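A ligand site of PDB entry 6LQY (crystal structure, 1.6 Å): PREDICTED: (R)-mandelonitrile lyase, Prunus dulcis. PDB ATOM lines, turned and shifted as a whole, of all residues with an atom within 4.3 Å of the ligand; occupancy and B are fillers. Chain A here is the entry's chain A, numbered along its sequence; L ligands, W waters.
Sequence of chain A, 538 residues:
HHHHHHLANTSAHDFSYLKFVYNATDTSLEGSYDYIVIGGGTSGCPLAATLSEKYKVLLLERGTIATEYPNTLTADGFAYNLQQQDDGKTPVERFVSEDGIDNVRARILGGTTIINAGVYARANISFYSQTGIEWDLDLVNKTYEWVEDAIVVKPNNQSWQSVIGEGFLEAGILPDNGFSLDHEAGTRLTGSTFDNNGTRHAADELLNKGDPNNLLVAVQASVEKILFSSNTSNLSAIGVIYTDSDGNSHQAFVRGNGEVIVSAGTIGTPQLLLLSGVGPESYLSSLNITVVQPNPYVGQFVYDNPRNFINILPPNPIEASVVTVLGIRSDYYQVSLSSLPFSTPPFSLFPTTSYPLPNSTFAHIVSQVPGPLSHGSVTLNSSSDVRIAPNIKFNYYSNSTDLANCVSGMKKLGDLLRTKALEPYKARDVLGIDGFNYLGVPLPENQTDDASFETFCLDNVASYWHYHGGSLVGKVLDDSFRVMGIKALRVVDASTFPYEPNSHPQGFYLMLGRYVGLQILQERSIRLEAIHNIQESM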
ATOM      1  N   ILE A  38      -2.282 -13.255  40.244  1.00  0.00           N
ATOM      2  CA  ILE A  38      -3.720 -13.305  39.963  1.00  0.00           C
ATOM      3  C   ILE A  38      -3.908 -13.964  38.616  1.00  0.00           C
ATOM      4  O   ILE A  38      -3.588 -13.374  37.576  1.00  0.00           O
ATOM      5  CB  ILE A  38      -4.328 -11.896  39.974  1.00  0.00           C
ATOM      6  CG1 ILE A  38      -4.086 -11.232  41.330  1.00  0.00           C
ATOM      7  CG2 ILE A  38      -5.825 -11.973  39.650  1.00  0.00           C
ATOM      8  CD1 ILE A  38      -4.151  -9.714  41.271  1.00  0.00           C
ATOM      9  N   GLY A  39      -4.436 -15.185  38.613  1.00  0.00           N
ATOM     10  CA  GLY A  39      -4.665 -15.902  37.365  1.00  0.00           C
ATOM     11  C   GLY A  39      -3.664 -17.039  37.188  1.00  0.00           C
ATOM     12  O   GLY A  39      -2.485 -16.796  36.895  1.00  0.00           O
ATOM     13  N   GLY A  40      -4.127 -18.275  37.370  1.00  0.00           N
ATOM     14  CA  GLY A  40      -3.254 -19.437  37.254  1.00  0.00           C
ATOM     15  C   GLY A  40      -3.254 -19.965  35.829  1.00  0.00           C
ATOM     16  O   GLY A  40      -3.641 -21.110  35.584  1.00  0.00           O
ATOM     17  N   GLY A  41      -2.827 -19.115  34.902  1.00  0.00           N
ATOM     18  CA  GLY A  41      -2.905 -19.455  33.489  1.00  0.00           C
ATOM     19  C   GLY A  41      -1.560 -19.630  32.822  1.00  0.00           C
ATOM     20  O   GLY A  41      -0.579 -20.027  33.456  1.00  0.00           O
ATOM     21  N   THR A  42      -1.520 -19.322  31.515  1.00  0.00           N
ATOM     22  CA  THR A  42      -0.349 -19.595  30.687  1.00  0.00           C
ATOM     23  C   THR A  42       0.904 -18.908  31.241  1.00  0.00           C
ATOM     24  O   THR A  42       1.948 -19.552  31.411  1.00  0.00           O
ATOM     25  CB  THR A  42      -0.637 -19.135  29.253  1.00  0.00           C
ATOM     26  OG1 THR A  42      -1.865 -19.737  28.830  1.00  0.00           O
ATOM     27  CG2 THR A  42       0.493 -19.554  28.289  1.00  0.00           C
ATOM     28  N   SER A  43       0.807 -17.609  31.527  1.00  0.00           N
ATOM     29  CA  SER A  43       1.936 -16.911  32.131  1.00  0.00           C
ATOM     30  C   SER A  43       1.962 -17.057  33.647  1.00  0.00           C
ATOM     31  O   SER A  43       3.049 -17.154  34.240  1.00  0.00           O
ATOM     32  CB  SER A  43       1.913 -15.415  31.774  1.00  0.00           C
ATOM     33  OG  SER A  43       2.144 -15.168  30.400  1.00  0.00           O
ATOM     34  N   LEU A  60      -3.731 -17.247  42.773  1.00  0.00           N
ATOM     35  CA  LEU A  60      -5.192 -17.236  42.866  1.00  0.00           C
ATOM     36  C   LEU A  60      -5.794 -17.490  41.483  1.00  0.00           C
ATOM     37  O   LEU A  60      -5.536 -16.729  40.552  1.00  0.00           O
ATOM     38  CB  LEU A  60      -5.689 -15.907  43.412  1.00  0.00           C
ATOM     39  CG  LEU A  60      -5.163 -15.598  44.810  1.00  0.00           C
ATOM     40  CD1 LEU A  60      -5.412 -14.137  45.201  1.00  0.00           C
ATOM     41  CD2 LEU A  60      -5.738 -16.546  45.853  1.00  0.00           C
ATOM     42  N   GLU A  61      -6.595 -18.538  41.374  1.00  0.00           N
ATOM     43  CA  GLU A  61      -7.242 -18.902  40.117  1.00  0.00           C
ATOM     44  C   GLU A  61      -8.751 -19.050  40.304  1.00  0.00           C
ATOM     45  O   GLU A  61      -9.194 -19.769  41.203  1.00  0.00           O
ATOM     46  CB  GLU A  61      -6.642 -20.196  39.561  1.00  0.00           C
ATOM     47  CG  GLU A  61      -7.485 -20.857  38.482  1.00  0.00           C
ATOM     48  CD  GLU A  61      -7.658 -19.982  37.240  1.00  0.00           C
ATOM     49  OE1 GLU A  61      -6.699 -19.279  36.844  1.00  0.00           O
ATOM     50  OE2 GLU A  61      -8.765 -19.989  36.676  1.00  0.00           O
ATOM     51  N   ARG A  62      -9.532 -18.412  39.433  1.00  0.00           N
ATOM     52  CA  ARG A  62     -10.986 -18.437  39.600  1.00  0.00           C
ATOM     53  C   ARG A  62     -11.610 -19.792  39.248  1.00  0.00           C
ATOM     54  O   ARG A  62     -12.697 -20.118  39.744  1.00  0.00           O
ATOM     55  CB  ARG A  62     -11.621 -17.325  38.760  1.00  0.00           C
ATOM     56  CG  ARG A  62     -11.444 -17.547  37.255  1.00  0.00           C
ATOM     57  CD  ARG A  62     -12.106 -16.448  36.386  1.00  0.00           C
ATOM     58  NE  ARG A  62     -11.956 -16.823  34.981  1.00  0.00           N
ATOM     59  CZ  ARG A  62     -12.806 -16.513  34.018  1.00  0.00           C
ATOM     60  NH1 ARG A  62     -13.888 -15.778  34.295  1.00  0.00           N
ATOM     61  NH2 ARG A  62     -12.591 -16.955  32.783  1.00  0.00           N
ATOM     62  N   VAL A 104     -14.134 -17.855  23.033  1.00  0.00           N
ATOM     63  CA  VAL A 104     -14.034 -18.497  24.342  1.00  0.00           C
ATOM     64  C   VAL A 104     -12.769 -18.032  25.047  1.00  0.00           C
ATOM     65  O   VAL A 104     -11.809 -17.589  24.416  1.00  0.00           O
ATOM     66  CB  VAL A 104     -14.031 -20.051  24.260  1.00  0.00           C
ATOM     67  CG1 VAL A 104     -15.291 -20.592  23.537  1.00  0.00           C
ATOM     68  CG2 VAL A 104     -12.767 -20.543  23.578  1.00  0.00           C
ATOM     69  N   ALA A 106     -10.443 -19.363  28.863  1.00  0.00           N
ATOM     70  CA  ALA A 106     -10.369 -20.451  29.818  1.00  0.00           C
ATOM     71  C   ALA A 106     -10.784 -20.008  31.222  1.00  0.00           C
ATOM     72  O   ALA A 106     -10.685 -18.835  31.591  1.00  0.00           O
ATOM     73  CB  ALA A 106      -8.958 -21.029  29.877  1.00  0.00           C
ATOM     74  N   ARG A 107     -11.208 -20.995  32.018  1.00  0.00           N
ATOM     75  CA  ARG A 107     -11.621 -20.776  33.406  1.00  0.00           C
ATOM     76  C   ARG A 107     -11.227 -22.044  34.169  1.00  0.00           C
ATOM     77  O   ARG A 107     -12.055 -22.886  34.510  1.00  0.00           O
ATOM     78  CB  ARG A 107     -13.126 -20.498  33.512  1.00  0.00           C
ATOM     79  CG  ARG A 107     -13.599 -20.103  34.912  1.00  0.00           C
ATOM     80  CD  ARG A 107     -15.078 -19.666  34.894  1.00  0.00           C
ATOM     81  NE  ARG A 107     -15.829 -20.600  34.071  1.00  0.00           N
ATOM     82  CZ  ARG A 107     -16.913 -20.344  33.356  1.00  0.00           C
ATOM     83  NH1 ARG A 107     -17.497 -19.130  33.316  1.00  0.00           N
ATOM     84  NH2 ARG A 107     -17.427 -21.335  32.657  1.00  0.00           N
ATOM     85  N   ILE A 108      -9.920 -22.191  34.433  1.00  0.00           N
ATOM     86  CA  ILE A 108      -9.386 -23.459  34.918  1.00  0.00           C
ATOM     87  C   ILE A 108      -7.925 -23.250  35.305  1.00  0.00           C
ATOM     88  O   ILE A 108      -7.242 -22.398  34.724  1.00  0.00           O
ATOM     89  CB  ILE A 108      -9.542 -24.558  33.852  1.00  0.00           C
ATOM     90  CG1 ILE A 108      -9.495 -25.959  34.480  1.00  0.00           C
ATOM     91  CG2 ILE A 108      -8.464 -24.408  32.779  1.00  0.00           C
ATOM     92  CD1 ILE A 108     -10.742 -26.292  35.307  1.00  0.00           C
ATOM     93  N   GLY A 111      -5.129 -22.344  32.865  1.00  0.00           N
ATOM     94  CA  GLY A 111      -5.559 -21.351  31.901  1.00  0.00           C
ATOM     95  C   GLY A 111      -5.803 -21.934  30.528  1.00  0.00           C
ATOM     96  O   GLY A 111      -6.282 -23.063  30.371  1.00  0.00           O
ATOM     97  N   THR A 112      -5.481 -21.136  29.507  1.00  0.00           N
ATOM     98  CA  THR A 112      -5.905 -21.512  28.172  1.00  0.00           C
ATOM     99  C   THR A 112      -5.080 -22.678  27.617  1.00  0.00           C
ATOM    100  O   THR A 112      -5.546 -23.386  26.712  1.00  0.00           O
ATOM    101  CB  THR A 112      -5.886 -20.243  27.298  1.00  0.00           C
ATOM    102  OG1 THR A 112      -6.838 -19.320  27.844  1.00  0.00           O
ATOM    103  CG2 THR A 112      -6.314 -20.562  25.864  1.00  0.00           C
ATOM    104  N   ILE A 115      -7.194 -25.881  27.385  1.00  0.00           N
ATOM    105  CA  ILE A 115      -8.313 -26.019  26.454  1.00  0.00           C
ATOM    106  C   ILE A 115      -7.905 -25.787  25.002  1.00  0.00           C
ATOM    107  O   ILE A 115      -8.769 -25.864  24.119  1.00  0.00           O
ATOM    108  CB  ILE A 115      -9.485 -25.075  26.826  1.00  0.00           C
ATOM    109  CG1 ILE A 115      -9.063 -23.602  26.721  1.00  0.00           C
ATOM    110  CG2 ILE A 115     -10.033 -25.407  28.211  1.00  0.00           C
ATOM    111  CD1 ILE A 115     -10.264 -22.607  26.712  1.00  0.00           C
ATOM    112  N   ASN A 116      -6.642 -25.496  24.729  1.00  0.00           N
ATOM    113  CA  ASN A 116      -6.265 -24.974  23.432  1.00  0.00           C
ATOM    114  C   ASN A 116      -5.903 -26.109  22.462  1.00  0.00           C
ATOM    115  O   ASN A 116      -6.082 -27.298  22.755  1.00  0.00           O
ATOM    116  CB  ASN A 116      -5.171 -23.913  23.599  1.00  0.00           C
ATOM    117  CG  ASN A 116      -3.815 -24.451  23.979  1.00  0.00           C
ATOM    118  OD1 ASN A 116      -3.567 -25.648  24.018  1.00  0.00           O
ATOM    119  ND2 ASN A 116      -2.908 -23.520  24.255  1.00  0.00           N
ATOM    120  N   ALA A 117      -5.426 -25.749  21.275  1.00  0.00           N
ATOM    121  CA  ALA A 117      -5.167 -26.735  20.225  1.00  0.00           C
ATOM    122  C   ALA A 117      -3.743 -27.302  20.287  1.00  0.00           C
ATOM    123  O   ALA A 117      -3.348 -28.066  19.393  1.00  0.00           O
ATOM    124  CB  ALA A 117      -5.460 -26.122  18.845  1.00  0.00           C
ATOM    125  N   GLY A 118      -2.969 -26.918  21.290  1.00  0.00           N
ATOM    126  CA  GLY A 118      -1.712 -27.597  21.574  1.00  0.00           C
ATOM    127  C   GLY A 118      -0.515 -27.166  20.757  1.00  0.00           C
ATOM    128  O   GLY A 118       0.591 -27.673  20.996  1.00  0.00           O
ATOM    129  N   VAL A 119      -0.672 -26.260  19.784  1.00  0.00           N
ATOM    130  CA  VAL A 119       0.431 -25.935  18.891  1.00  0.00           C
ATOM    131  C   VAL A 119       1.492 -25.159  19.666  1.00  0.00           C
ATOM    132  O   VAL A 119       1.178 -24.181  20.357  1.00  0.00           O
ATOM    133  CB  VAL A 119      -0.071 -25.119  17.690  1.00  0.00           C
ATOM    134  CG1 VAL A 119       1.071 -24.890  16.694  1.00  0.00           C
ATOM    135  CG2 VAL A 119      -1.237 -25.814  17.037  1.00  0.00           C
ATOM    136  N   ALA A 221     -11.020 -19.128  43.325  1.00  0.00           N
ATOM    137  CA  ALA A 221     -10.705 -17.846  43.964  1.00  0.00           C
ATOM    138  C   ALA A 221     -10.951 -16.757  42.934  1.00  0.00           C
ATOM    139  O   ALA A 221     -10.143 -16.555  42.018  1.00  0.00           O
ATOM    140  CB  ALA A 221      -9.260 -17.822  44.458  1.00  0.00           C
ATOM    141  N   SER A 222     -12.068 -16.045  43.068  1.00  0.00           N
ATOM    142  CA  SER A 222     -12.428 -14.984  42.118  1.00  0.00           C
ATOM    143  C   SER A 222     -11.878 -13.660  42.659  1.00  0.00           C
ATOM    144  O   SER A 222     -12.397 -13.114  43.624  1.00  0.00           O
ATOM    145  CB  SER A 222     -13.940 -14.971  41.949  1.00  0.00           C
ATOM    146  OG  SER A 222     -14.392 -13.800  41.300  1.00  0.00           O
ATOM    147  N   VAL A 223     -10.788 -13.182  42.064  1.00  0.00           N
ATOM    148  CA  VAL A 223     -10.163 -11.943  42.535  1.00  0.00           C
ATOM    149  C   VAL A 223     -10.978 -10.749  42.032  1.00  0.00           C
ATOM    150  O   VAL A 223     -11.086 -10.532  40.817  1.00  0.00           O
ATOM    151  CB  VAL A 223      -8.700 -11.846  42.087  1.00  0.00           C
ATOM    152  CG1 VAL A 223      -8.097 -10.539  42.617  1.00  0.00           C
ATOM    153  CG2 VAL A 223      -7.924 -13.048  42.631  1.00  0.00           C
ATOM    154  N   SER A 263      -2.117 -11.653  36.058  1.00  0.00           N
ATOM    155  CA  SER A 263      -1.918 -12.599  34.962  1.00  0.00           C
ATOM    156  C   SER A 263      -3.267 -13.185  34.553  1.00  0.00           C
ATOM    157  O   SER A 263      -3.395 -14.369  34.258  1.00  0.00           O
ATOM    158  CB  SER A 263      -0.928 -13.694  35.366  1.00  0.00           C
ATOM    159  OG  SER A 263       0.347 -13.125  35.657  1.00  0.00           O
ATOM    160  N   ALA A 264      -4.296 -12.326  34.532  1.00  0.00           N
ATOM    161  CA  ALA A 264      -5.664 -12.752  34.320  1.00  0.00           C
ATOM    162  C   ALA A 264      -6.099 -12.736  32.851  1.00  0.00           C
ATOM    163  O   ALA A 264      -7.285 -12.940  32.563  1.00  0.00           O
ATOM    164  CB  ALA A 264      -6.621 -11.879  35.154  1.00  0.00           C
ATOM    165  N   GLY A 265      -5.156 -12.539  31.924  1.00  0.00           N
ATOM    166  CA  GLY A 265      -5.426 -12.640  30.513  1.00  0.00           C
ATOM    167  C   GLY A 265      -5.862 -11.317  29.887  1.00  0.00           C
ATOM    168  O   GLY A 265      -6.105 -10.318  30.552  1.00  0.00           O
ATOM    169  N   GLY A 268      -9.288 -10.654  31.432  1.00  0.00           N
ATOM    170  CA  GLY A 268      -9.375 -10.528  32.880  1.00  0.00           C
ATOM    171  C   GLY A 268      -8.499  -9.447  33.470  1.00  0.00           C
ATOM    172  O   GLY A 268      -8.856  -8.832  34.476  1.00  0.00           O
ATOM    173  N   VAL A 386     -16.896  -9.042  39.284  1.00  0.00           N
ATOM    174  CA  VAL A 386     -15.879  -9.558  38.372  1.00  0.00           C
ATOM    175  C   VAL A 386     -16.332 -10.821  37.666  1.00  0.00           C
ATOM    176  O   VAL A 386     -15.731 -11.223  36.657  1.00  0.00           O
ATOM    177  CB  VAL A 386     -14.544  -9.782  39.123  1.00  0.00           C
ATOM    178  CG1 VAL A 386     -14.610 -11.075  39.919  1.00  0.00           C
ATOM    179  CG2 VAL A 386     -13.390  -9.817  38.142  1.00  0.00           C
ATOM    180  N   TRP A 465      -8.587 -17.014  18.221  1.00  0.00           N
ATOM    181  CA  TRP A 465      -8.486 -17.267  19.647  1.00  0.00           C
ATOM    182  C   TRP A 465      -7.190 -16.712  20.215  1.00  0.00           C
ATOM    183  O   TRP A 465      -6.899 -16.920  21.419  1.00  0.00           O
ATOM    184  CB  TRP A 465      -8.562 -18.763  19.973  1.00  0.00           C
ATOM    185  CG  TRP A 465      -9.819 -19.474  19.570  1.00  0.00           C
ATOM    186  CD1 TRP A 465     -11.087 -19.117  19.888  1.00  0.00           C
ATOM    187  CD2 TRP A 465      -9.914 -20.710  18.844  1.00  0.00           C
ATOM    188  NE1 TRP A 465     -11.991 -20.032  19.365  1.00  0.00           N
ATOM    189  CE2 TRP A 465     -11.282 -21.022  18.730  1.00  0.00           C
ATOM    190  CE3 TRP A 465      -8.977 -21.570  18.271  1.00  0.00           C
ATOM    191  CZ2 TRP A 465     -11.739 -22.157  18.060  1.00  0.00           C
ATOM    192  CZ3 TRP A 465      -9.426 -22.707  17.603  1.00  0.00           C
ATOM    193  CH2 TRP A 465     -10.798 -22.988  17.499  1.00  0.00           C
ATOM    194  N   HIS A 466      -6.409 -15.993  19.421  1.00  0.00           N
ATOM    195  CA  HIS A 466      -5.094 -15.508  19.840  1.00  0.00           C
ATOM    196  C   HIS A 466      -5.138 -14.038  20.188  1.00  0.00           C
ATOM    197  O   HIS A 466      -4.228 -13.266  19.866  1.00  0.00           O
ATOM    198  CB  HIS A 466      -4.063 -15.781  18.753  1.00  0.00           C
ATOM    199  CG  HIS A 466      -3.839 -17.239  18.466  1.00  0.00           C
ATOM    200  ND1 HIS A 466      -2.927 -17.671  17.519  1.00  0.00           N
ATOM    201  CD2 HIS A 466      -4.379 -18.352  19.012  1.00  0.00           C
ATOM    202  CE1 HIS A 466      -2.944 -18.994  17.477  1.00  0.00           C
ATOM    203  NE2 HIS A 466      -3.808 -19.432  18.375  1.00  0.00           N
ATOM    204  N   ASP A 493       1.025 -11.454  30.973  1.00  0.00           N
ATOM    205  CA  ASP A 493       0.096 -12.322  30.244  1.00  0.00           C
ATOM    206  C   ASP A 493      -0.076 -11.734  28.843  1.00  0.00           C
ATOM    207  O   ASP A 493       0.674 -10.831  28.463  1.00  0.00           O
ATOM    208  CB  ASP A 493      -1.246 -12.465  30.973  1.00  0.00           C
ATOM    209  CG  ASP A 493      -1.949 -11.124  31.201  1.00  0.00           C
ATOM    210  OD1 ASP A 493      -1.666 -10.157  30.476  1.00  0.00           O
ATOM    211  OD2 ASP A 493      -2.802 -11.067  32.124  1.00  0.00           O
ATOM    212  N   ALA A 494      -1.052 -12.218  28.082  1.00  0.00           N
ATOM    213  CA  ALA A 494      -1.182 -11.738  26.716  1.00  0.00           C
ATOM    214  C   ALA A 494      -1.806 -10.350  26.598  1.00  0.00           C
ATOM    215  O   ALA A 494      -1.933  -9.835  25.481  1.00  0.00           O
ATOM    216  CB  ALA A 494      -1.981 -12.754  25.895  1.00  0.00           C
ATOM    217  N   HIS A 504       1.400 -18.839  16.902  1.00  0.00           N
ATOM    218  CA  HIS A 504       0.793 -19.598  17.986  1.00  0.00           C
ATOM    219  C   HIS A 504       1.519 -19.170  19.260  1.00  0.00           C
ATOM    220  O   HIS A 504       2.643 -19.629  19.521  1.00  0.00           O
ATOM    221  CB  HIS A 504       0.889 -21.103  17.741  1.00  0.00           C
ATOM    222  CG  HIS A 504       0.024 -21.573  16.609  1.00  0.00           C
ATOM    223  ND1 HIS A 504       0.416 -21.502  15.283  1.00  0.00           N
ATOM    224  CD2 HIS A 504      -1.235 -22.065  16.595  1.00  0.00           C
ATOM    225  CE1 HIS A 504      -0.555 -21.950  14.510  1.00  0.00           C
ATOM    226  NE2 HIS A 504      -1.571 -22.305  15.285  1.00  0.00           N
ATOM    227  N   PRO A 505       0.911 -18.303  20.068  1.00  0.00           N
ATOM    228  CA  PRO A 505       1.657 -17.562  21.084  1.00  0.00           C
ATOM    229  C   PRO A 505       1.807 -18.241  22.437  1.00  0.00           C
ATOM    230  O   PRO A 505       2.452 -17.644  23.299  1.00  0.00           O
ATOM    231  CB  PRO A 505       0.805 -16.288  21.238  1.00  0.00           C
ATOM    232  CG  PRO A 505      -0.596 -16.765  20.978  1.00  0.00           C
ATOM    233  CD  PRO A 505      -0.442 -17.756  19.844  1.00  0.00           C
ATOM    234  N   GLN A 506       1.237 -19.435  22.677  1.00  0.00           N
ATOM    235  CA  GLN A 506       1.313 -20.002  24.023  1.00  0.00           C
ATOM    236  C   GLN A 506       2.764 -20.197  24.434  1.00  0.00           C
ATOM    237  O   GLN A 506       3.114 -19.943  25.590  1.00  0.00           O
ATOM    238  CB  GLN A 506       0.518 -21.312  24.142  1.00  0.00           C
ATOM    239  CG  GLN A 506       1.129 -22.568  23.524  1.00  0.00           C
ATOM    240  CD  GLN A 506       0.510 -23.871  24.061  1.00  0.00           C
ATOM    241  OE1 GLN A 506      -0.027 -23.909  25.167  1.00  0.00           O
ATOM    242  NE2 GLN A 506       0.553 -24.930  23.252  1.00  0.00           N
HETATM  243  P1  LIG L   1      -4.888 -17.542  30.280  1.00  0.00           P
HETATM  244  O1  LIG L   1      -6.294 -17.605  29.892  1.00  0.00           O
HETATM  245  O2  LIG L   1      -4.046 -18.698  30.005  1.00  0.00           O
HETATM  246  O3  LIG L   1      -4.809 -17.258  31.834  1.00  0.00           O
HETATM  247  C1  LIG L   1      -5.641 -16.338  32.537  1.00  0.00           C
HETATM  248  C2  LIG L   1      -6.156 -17.003  33.787  1.00  0.00           C
HETATM  249  O4  LIG L   1      -6.704 -16.048  34.721  1.00  0.00           O
HETATM  250  C3  LIG L   1      -7.270 -18.030  33.549  1.00  0.00           C
HETATM  251  O5  LIG L   1      -6.918 -19.283  34.095  1.00  0.00           O
HETATM  252  C4  LIG L   1      -8.491 -17.411  34.221  1.00  0.00           C
HETATM  253  O6  LIG L   1      -9.408 -18.362  34.690  1.00  0.00           O
HETATM  254  C5  LIG L   1      -7.861 -16.564  35.316  1.00  0.00           C
HETATM  255  N1  LIG L   1      -8.617 -15.445  35.786  1.00  0.00           N
HETATM  256  C6  LIG L   1      -9.180 -14.464  35.037  1.00  0.00           C
HETATM  257  N2  LIG L   1      -9.722 -13.510  35.728  1.00  0.00           N
HETATM  258  C7  LIG L   1      -9.492 -13.874  37.036  1.00  0.00           C
HETATM  259  C8  LIG L   1      -9.835 -13.281  38.265  1.00  0.00           C
HETATM  260  N3  LIG L   1     -10.467 -12.136  38.368  1.00  0.00           N
HETATM  261  N4  LIG L   1      -9.454 -13.935  39.387  1.00  0.00           N
HETATM  262  C9  LIG L   1      -8.808 -15.084  39.273  1.00  0.00           C
HETATM  263  N5  LIG L   1      -8.426 -15.723  38.174  1.00  0.00           N
HETATM  264  C10 LIG L   1      -8.806 -15.069  37.082  1.00  0.00           C
HETATM  265  N6  LIG L   1      -2.054 -20.688  21.269  1.00  0.00           N
HETATM  266  C11 LIG L   1      -1.092 -21.486  20.807  1.00  0.00           C
HETATM  267  O7  LIG L   1       0.079 -21.152  20.805  1.00  0.00           O
HETATM  268  N7  LIG L   1      -1.379 -22.700  20.273  1.00  0.00           N
HETATM  269  C12 LIG L   1      -2.670 -23.143  20.109  1.00  0.00           C
HETATM  270  O8  LIG L   1      -2.863 -24.221  19.647  1.00  0.00           O
HETATM  271  C13 LIG L   1      -3.705 -22.348  20.653  1.00  0.00           C
HETATM  272  N8  LIG L   1      -4.931 -22.764  20.581  1.00  0.00           N
HETATM  273  C14 LIG L   1      -5.892 -22.036  21.200  1.00  0.00           C
HETATM  274  C15 LIG L   1      -7.213 -22.516  21.218  1.00  0.00           C
HETATM  275  C16 LIG L   1      -8.215 -21.877  21.911  1.00  0.00           C
HETATM  276  C17 LIG L   1      -9.610 -22.436  21.946  1.00  0.00           C
HETATM  277  C18 LIG L   1      -7.907 -20.673  22.565  1.00  0.00           C
HETATM  278  C19 LIG L   1      -8.985 -19.935  23.311  1.00  0.00           C
HETATM  279  C20 LIG L   1      -6.647 -20.132  22.460  1.00  0.00           C
HETATM  280  C21 LIG L   1      -5.607 -20.819  21.838  1.00  0.00           C
HETATM  281  N9  LIG L   1      -4.295 -20.337  21.787  1.00  0.00           N
HETATM  282  C22 LIG L   1      -3.301 -21.096  21.233  1.00  0.00           C
HETATM  283  C23 LIG L   1      -3.949 -19.050  22.404  1.00  0.00           C
HETATM  284  C24 LIG L   1      -3.143 -19.167  23.665  1.00  0.00           C
HETATM  285  O9  LIG L   1      -3.452 -20.358  24.299  1.00  0.00           O
HETATM  286  C25 LIG L   1      -3.482 -17.953  24.543  1.00  0.00           C
HETATM  287  O10 LIG L   1      -3.277 -16.760  23.862  1.00  0.00           O
HETATM  288  C26 LIG L   1      -2.713 -17.879  25.858  1.00  0.00           C
HETATM  289  O11 LIG L   1      -2.833 -19.153  26.478  1.00  0.00           O
HETATM  290  C27 LIG L   1      -3.187 -16.792  26.792  1.00  0.00           C
HETATM  291  O12 LIG L   1      -2.450 -16.829  28.036  1.00  0.00           O
HETATM  292  P2  LIG L   1      -2.795 -15.842  29.239  1.00  0.00           P
HETATM  293  O13 LIG L   1      -1.918 -16.156  30.374  1.00  0.00           O
HETATM  294  O14 LIG L   1      -2.830 -14.495  28.688  1.00  0.00           O
HETATM  295  O15 LIG L   1      -4.264 -16.281  29.593  1.00  0.00           O
HETATM  296  O   HOH W   1      -5.109 -14.775  24.580  1.00  0.00           O
HETATM  297  O   HOH W   2      -8.927 -16.900  30.678  1.00  0.00           O
HETATM  298  O   HOH W   3      -5.134 -13.872  27.269  1.00  0.00           O
HETATM  299  O   HOH W   4     -10.717 -10.066  36.246  1.00  0.00           O
HETATM  300  O   HOH W   5      -7.151 -15.560  27.974  1.00  0.00           O
HETATM  301  O   HOH W   6       3.006 -21.805  20.938  1.00  0.00           O
HETATM  302  O   HOH W   7      -4.928 -22.023  17.532  1.00  0.00           O
HETATM  303  O   HOH W   8      -1.873 -16.474  33.147  1.00  0.00           O
HETATM  304  O   HOH W   9      -2.458 -14.327  22.472  1.00  0.00           O
HETATM  305  O   HOH W  10     -12.184 -12.337  34.683  1.00  0.00           O
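The backbone NH of Thr 42 sits at hydrogen-bond distance from an oxygen (O2) of the ligand (3.0 Å).
The side-chain hydroxyl (OG1) of Thr 42 sits at hydrogen-bond distance from an oxygen (O11) of the ligand, 2.6 Å away.
OE2 of Glu 61 lies within hydrogen-bond range of O6 of the ligand (2.6 Å).
The backbone NH (N) of Thr 112 is in hydrogen-bond range of an oxygen (O2) of the ligand.
The side-chain hydroxyl of Thr 112 sits at hydrogen-bond distance from an oxygen (O1) of the ligand, at 2.7 Å.
N of Gln 506 lies within hydrogen-bond range of O7 of the ligand (2.8 Å).
The backbone NH (N) of Ala 494 is in hydrogen-bond range of an oxygen (O14) of the ligand.
The backbone NH (N) of Val 119 sits at hydrogen-bond distance from an oxygen (O8) of the ligand (3.0 Å).
The backbone carbonyl oxygen (O) of Val 119 is in hydrogen-bond range of a nitrogen (N7) of the ligand, at 3.0 Å.
N of Arg 62 sits at hydrogen-bond distance from N5 of the ligand, at 3.2 Å.
NE of Arg 62 sits at hydrogen-bond distance from O6 of the ligand, 3.0 Å away.
N of Val 223 is in hydrogen-bond range of N4 of the ligand (3.1 Å).
A nitrogen (N3) of the ligand is in hydrogen-bond range of the backbone carbonyl oxygen of Val 223 (3.0 Å).
A nitrogen (N8) of the ligand is in hydrogen-bond range of the backbone NH (N) of Ala 117, 3.1 Å away.
ND2 of Asn 116 sits at hydrogen-bond distance from O9 of the ligand (3.2 Å).
The backbone NH of Gly 118 sits at hydrogen-bond distance from an oxygen (O8) of the ligand (3.2 Å).
O of Ile 108 is in hydrogen-bond range of O5 of the ligand (3.2 Å).
N of Ser 43 sits at hydrogen-bond distance from O13 of the ligand (3.3 Å).
The backbone carbonyl oxygen of Ala 106 lies within hydrogen-bond range of an oxygen (O6) of the ligand (3.4 Å).
N of Ala 221 sits at hydrogen-bond distance from O of Glu 61, 2.9 Å away.
OE1 of Gln 506 is in hydrogen-bond range of ND2 of Asn 116, 3.0 Å away.
NH2 of Arg 62 lies within hydrogen-bond range of O of Ala 106.
N of Gly 118 lies within hydrogen-bond range of OD1 of Asn 116 (3.1 Å).
O of Leu 60 sits at hydrogen-bond distance from N of Gly 39 (2.7 Å).
OD2 of Asp 493 sits at hydrogen-bond distance from N of Gly 265 (2.8 Å).
N of Ser 263 sits at hydrogen-bond distance from O of Ile 38 (2.7 Å).
The backbone carbonyl oxygen (O) of Ile 38 is in hydrogen-bond range of the backbone NH (N) of Ala 264, at 3.3 Å.
The backbone carbonyl oxygen (O) of His 504 lies close to an oxygen (O7) of the ligand (3.2 Å).
The backbone nitrogen of Pro 505 lies close to an oxygen (O7) of the ligand (3.1 Å).
Merely in contact with the ligand: Gly 39, Gly 41, Leu 60, Val 104, Arg 107, Gly 111, Ala 221, Ser 263, Ala 264, Gly 265, Val 386, Trp 465, His 466 and Asp 493.
Hydrophobic or aromatic side chains that line the ligand: Val 104, Ala 117, Val 119, Val 223, Ala 264, Val 386, Trp 465, His 466, Ala 494, His 504 and Pro 505.
Of the 35 residues printed, 30 come within 4 Å of the ligand.
The nearest printed residue that does not touch the ligand is Gly 40 (4.04 Å).
Water W2 lies within hydrogen-bond range of the backbone carbonyl oxygen of Ala 106 (2.8 Å) and an oxygen (O1) of the ligand (2.8 Å).
Water W9 bridges O10 of the ligand and O of His 466.
Water W4 bridges O of Gly 268 (2.8 Å) and N3 of the ligand (3.0 Å).
Water W7 lies within hydrogen-bond range of a ring nitrogen (NE2) of His 466 and a nitrogen (N8) of the ligand.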
